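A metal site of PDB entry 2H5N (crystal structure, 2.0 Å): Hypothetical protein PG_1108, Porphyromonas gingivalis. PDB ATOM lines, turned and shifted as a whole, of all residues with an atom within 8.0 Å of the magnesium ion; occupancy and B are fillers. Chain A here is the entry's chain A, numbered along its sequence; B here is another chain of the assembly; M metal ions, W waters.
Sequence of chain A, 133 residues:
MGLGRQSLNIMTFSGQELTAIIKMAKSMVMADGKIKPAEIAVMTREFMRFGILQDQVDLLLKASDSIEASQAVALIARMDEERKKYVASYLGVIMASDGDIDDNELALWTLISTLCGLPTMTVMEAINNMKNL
Of the 17 residues printed, 3 come within 4 Å of the magnesium ion.
The nearest printed residue that does not touch the magnesium ion is Glu 39 (4.4 Å).
Water W2 lies within hydrogen-bond range of the side-chain carboxylate of Glu 39 and the backbone NH of Lys 36.
The magnesium ion is bound by the side-chain carboxylate of Asp 32 (2.1 Å), the backbone carbonyl oxygen of Lys 34 (2.3 Å) and the backbone carbonyl oxygen of Val 29 (2.4 Å).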
ATOM      1  N   LYS A  26     -14.953  19.639  12.399  1.00  0.00           N
ATOM      2  CA  LYS A  26     -13.803  19.997  13.230  1.00  0.00           C
ATOM      3  C   LYS A  26     -13.715  19.229  14.582  1.00  0.00           C
ATOM      4  O   LYS A  26     -12.645  18.725  14.969  1.00  0.00           O
ATOM      5  CB  LYS A  26     -13.798  21.484  13.465  1.00  0.00           C
ATOM      6  CG  LYS A  26     -13.129  22.310  12.341  1.00  0.00           C
ATOM      7  CD  LYS A  26     -13.265  23.806  12.648  1.00  0.00           C
ATOM      8  CE  LYS A  26     -12.640  24.629  11.585  1.00  0.00           C
ATOM      9  NZ  LYS A  26     -12.404  26.077  11.966  1.00  0.00           N
ATOM     10  N   SER A  27     -14.814  19.196  15.307  1.00  0.00           N
ATOM     11  CA  SER A  27     -14.840  18.574  16.609  1.00  0.00           C
ATOM     12  C   SER A  27     -14.503  17.101  16.474  1.00  0.00           C
ATOM     13  O   SER A  27     -13.713  16.560  17.244  1.00  0.00           O
ATOM     14  CB  SER A  27     -16.209  18.762  17.280  1.00  0.00           C
ATOM     15  OG  SER A  27     -16.614  20.120  17.263  1.00  0.00           O
ATOM     16  N   MET A  28     -15.113  16.440  15.482  1.00  0.00           N
ATOM     17  CA  MET A  28     -14.873  14.998  15.251  1.00  0.00           C
ATOM     18  C   MET A  28     -13.399  14.704  14.959  1.00  0.00           C
ATOM     19  O   MET A  28     -12.817  13.838  15.632  1.00  0.00           O
ATOM     20  CB  MET A  28     -15.810  14.440  14.167  1.00  0.00           C
ATOM     21  CG  MET A  28     -15.698  12.932  13.827  1.00  0.00           C
ATOM     22  SD  MET A  28     -16.798  12.366  12.504  1.00  0.00           S
ATOM     23  CE  MET A  28     -16.048  13.234  11.124  1.00  0.00           C
ATOM     24  N   VAL A  29     -12.790  15.460  14.025  1.00  0.00           N
ATOM     25  CA  VAL A  29     -11.389  15.240  13.614  1.00  0.00           C
ATOM     26  C   VAL A  29     -10.336  15.688  14.656  1.00  0.00           C
ATOM     27  O   VAL A  29      -9.227  15.165  14.661  1.00  0.00           O
ATOM     28  CB  VAL A  29     -10.986  15.875  12.181  1.00  0.00           C
ATOM     29  CG1 VAL A  29     -11.808  15.300  11.049  1.00  0.00           C
ATOM     30  CG2 VAL A  29     -11.090  17.368  12.157  1.00  0.00           C
ATOM     31  N   MET A  30     -10.667  16.657  15.508  1.00  0.00           N
ATOM     32  CA  MET A  30      -9.750  17.035  16.599  1.00  0.00           C
ATOM     33  C   MET A  30      -9.828  16.061  17.765  1.00  0.00           C
ATOM     34  O   MET A  30      -8.958  16.088  18.643  1.00  0.00           O
ATOM     35  CB  MET A  30     -10.026  18.440  17.139  1.00  0.00           C
ATOM     36  CG  MET A  30     -10.108  19.521  16.061  1.00  0.00           C
ATOM     37  SD  MET A  30      -9.937  21.222  16.651  1.00  0.00           S
ATOM     38  CE  MET A  30      -8.136  21.106  16.847  1.00  0.00           C
ATOM     39  N   ALA A  31     -10.848  15.212  17.809  1.00  0.00           N
ATOM     40  CA  ALA A  31     -11.076  14.455  19.051  1.00  0.00           C
ATOM     41  C   ALA A  31      -9.852  13.690  19.546  1.00  0.00           C
ATOM     42  O   ALA A  31      -9.538  13.710  20.730  1.00  0.00           O
ATOM     43  CB  ALA A  31     -12.285  13.526  18.950  1.00  0.00           C
ATOM     44  N   ASP A  32      -9.138  13.028  18.645  1.00  0.00           N
ATOM     45  CA  ASP A  32      -7.971  12.262  19.060  1.00  0.00           C
ATOM     46  C   ASP A  32      -6.680  13.073  19.194  1.00  0.00           C
ATOM     47  O   ASP A  32      -5.622  12.519  19.453  1.00  0.00           O
ATOM     48  CB  ASP A  32      -7.811  11.038  18.158  1.00  0.00           C
ATOM     49  CG  ASP A  32      -7.195  11.357  16.826  1.00  0.00           C
ATOM     50  OD1 ASP A  32      -7.204  12.532  16.375  1.00  0.00           O
ATOM     51  OD2 ASP A  32      -6.699  10.396  16.227  1.00  0.00           O
ATOM     52  N   GLY A  33      -6.781  14.396  19.003  1.00  0.00           N
ATOM     53  CA  GLY A  33      -5.700  15.334  19.303  1.00  0.00           C
ATOM     54  C   GLY A  33      -4.580  15.339  18.291  1.00  0.00           C
ATOM     55  O   GLY A  33      -3.508  15.925  18.516  1.00  0.00           O
ATOM     56  N   LYS A  34      -4.818  14.668  17.162  1.00  0.00           N
ATOM     57  CA  LYS A  34      -3.815  14.536  16.110  1.00  0.00           C
ATOM     58  C   LYS A  34      -4.284  15.181  14.839  1.00  0.00           C
ATOM     59  O   LYS A  34      -5.473  15.170  14.535  1.00  0.00           O
ATOM     60  CB  LYS A  34      -3.522  13.050  15.866  1.00  0.00           C
ATOM     61  CG  LYS A  34      -2.658  12.437  16.962  1.00  0.00           C
ATOM     62  CD  LYS A  34      -2.942  10.958  17.175  1.00  0.00           C
ATOM     63  CE  LYS A  34      -2.224  10.096  16.178  1.00  0.00           C
ATOM     64  NZ  LYS A  34      -2.635   8.676  16.307  1.00  0.00           N
ATOM     65  N   ILE A  35      -3.380  15.756  14.057  1.00  0.00           N
ATOM     66  CA  ILE A  35      -3.823  16.265  12.738  1.00  0.00           C
ATOM     67  C   ILE A  35      -3.416  15.357  11.573  1.00  0.00           C
ATOM     68  O   ILE A  35      -2.244  15.036  11.404  1.00  0.00           O
ATOM     69  CB  ILE A  35      -3.411  17.727  12.482  1.00  0.00           C
ATOM     70  CG1 ILE A  35      -1.927  17.961  12.751  1.00  0.00           C
ATOM     71  CG2 ILE A  35      -4.280  18.655  13.347  1.00  0.00           C
ATOM     72  CD1 ILE A  35      -1.334  19.180  11.990  1.00  0.00           C
ATOM     73  N   LYS A  36      -4.416  14.924  10.810  1.00  0.00           N
ATOM     74  CA  LYS A  36      -4.229  14.193   9.550  1.00  0.00           C
ATOM     75  C   LYS A  36      -4.664  15.092   8.393  1.00  0.00           C
ATOM     76  O   LYS A  36      -5.866  15.207   8.107  1.00  0.00           O
ATOM     77  CB  LYS A  36      -5.014  12.881   9.555  1.00  0.00           C
ATOM     78  CG  LYS A  36      -4.583  11.839  10.647  1.00  0.00           C
ATOM     79  CD  LYS A  36      -5.402  10.520  10.606  1.00  0.00           C
ATOM     80  CE  LYS A  36      -4.853   9.512   9.581  1.00  0.00           C
ATOM     81  NZ  LYS A  36      -5.724   8.311   9.370  1.00  0.00           N
ATOM     82  N   GLU A  39      -7.556  13.971   6.024  1.00  0.00           N
ATOM     83  CA  GLU A  39      -8.924  14.091   6.559  1.00  0.00           C
ATOM     84  C   GLU A  39      -9.471  15.544   6.438  1.00  0.00           C
ATOM     85  O   GLU A  39     -10.652  15.752   6.115  1.00  0.00           O
ATOM     86  CB  GLU A  39      -8.940  13.698   8.026  1.00  0.00           C
ATOM     87  CG  GLU A  39      -8.986  12.188   8.300  1.00  0.00           C
ATOM     88  CD  GLU A  39      -9.030  11.839   9.793  1.00  0.00           C
ATOM     89  OE1 GLU A  39      -9.037  12.747  10.688  1.00  0.00           O
ATOM     90  OE2 GLU A  39      -9.039  10.625  10.082  1.00  0.00           O
ATOM     91  N   ILE A  40      -8.614  16.506   6.733  1.00  0.00           N
ATOM     92  CA  ILE A  40      -8.929  17.945   6.630  1.00  0.00           C
ATOM     93  C   ILE A  40      -9.255  18.398   5.178  1.00  0.00           C
ATOM     94  O   ILE A  40     -10.185  19.182   4.958  1.00  0.00           O
ATOM     95  CB  ILE A  40      -7.817  18.837   7.246  1.00  0.00           C
ATOM     96  CG1 ILE A  40      -7.436  18.364   8.664  1.00  0.00           C
ATOM     97  CG2 ILE A  40      -8.208  20.336   7.188  1.00  0.00           C
ATOM     98  CD1 ILE A  40      -8.629  18.236   9.625  1.00  0.00           C
ATOM     99  N   MET A  95     -13.460  10.625   7.561  1.00  0.00           N
ATOM    100  CA  MET A  95     -12.430   9.769   8.131  1.00  0.00           C
ATOM    101  C   MET A  95     -12.199   8.464   7.356  1.00  0.00           C
ATOM    102  O   MET A  95     -11.304   7.700   7.685  1.00  0.00           O
ATOM    103  CB  MET A  95     -12.638   9.568   9.650  1.00  0.00           C
ATOM    104  CG  MET A  95     -12.537  10.874  10.498  1.00  0.00           C
ATOM    105  SD  MET A  95     -12.711  10.504  12.231  1.00  0.00           S
ATOM    106  CE  MET A  95     -14.316   9.753  12.151  1.00  0.00           C
ATOM    107  N   GLU A 105     -12.462   5.428  14.619  1.00  0.00           N
ATOM    108  CA  GLU A 105     -13.118   6.382  13.741  1.00  0.00           C
ATOM    109  C   GLU A 105     -14.618   6.133  13.630  1.00  0.00           C
ATOM    110  O   GLU A 105     -15.406   7.069  13.690  1.00  0.00           O
ATOM    111  CB  GLU A 105     -12.494   6.315  12.353  1.00  0.00           C
ATOM    112  CG  GLU A 105     -11.347   7.229  12.212  1.00  0.00           C
ATOM    113  CD  GLU A 105     -10.119   6.596  11.563  1.00  0.00           C
ATOM    114  OE1 GLU A 105     -10.244   5.981  10.472  1.00  0.00           O
ATOM    115  OE2 GLU A 105      -9.024   6.742  12.170  1.00  0.00           O
ATOM    116  N   LEU A 108     -16.206   7.327  16.769  1.00  0.00           N
ATOM    117  CA  LEU A 108     -16.313   8.777  16.859  1.00  0.00           C
ATOM    118  C   LEU A 108     -17.456   9.321  16.011  1.00  0.00           C
ATOM    119  O   LEU A 108     -18.185  10.246  16.442  1.00  0.00           O
ATOM    120  CB  LEU A 108     -15.015   9.455  16.436  1.00  0.00           C
ATOM    121  CG  LEU A 108     -13.842   9.360  17.408  1.00  0.00           C
ATOM    122  CD1 LEU A 108     -12.552   9.835  16.705  1.00  0.00           C
ATOM    123  CD2 LEU A 108     -14.133  10.156  18.651  1.00  0.00           C
ATOM    124  N   ILE B  35      -8.065  24.013  14.330  1.00  0.00           N
ATOM    125  CA  ILE B  35      -7.645  23.642  12.973  1.00  0.00           C
ATOM    126  C   ILE B  35      -8.110  24.766  12.070  1.00  0.00           C
ATOM    127  O   ILE B  35      -9.284  25.124  12.119  1.00  0.00           O
ATOM    128  CB  ILE B  35      -8.327  22.332  12.505  1.00  0.00           C
ATOM    129  CG1 ILE B  35      -7.927  21.165  13.399  1.00  0.00           C
ATOM    130  CG2 ILE B  35      -8.035  22.009  11.013  1.00  0.00           C
ATOM    131  CD1 ILE B  35      -8.786  19.940  13.214  1.00  0.00           C
HETATM  132 MG    MG M   1      -7.278  13.707  14.630  1.00  0.00          MG
HETATM  133  O   HOH W   1     -10.179  12.531  15.660  1.00  0.00           O
HETATM  134  O   HOH W   2      -7.367  14.709  11.618  1.00  0.00           O
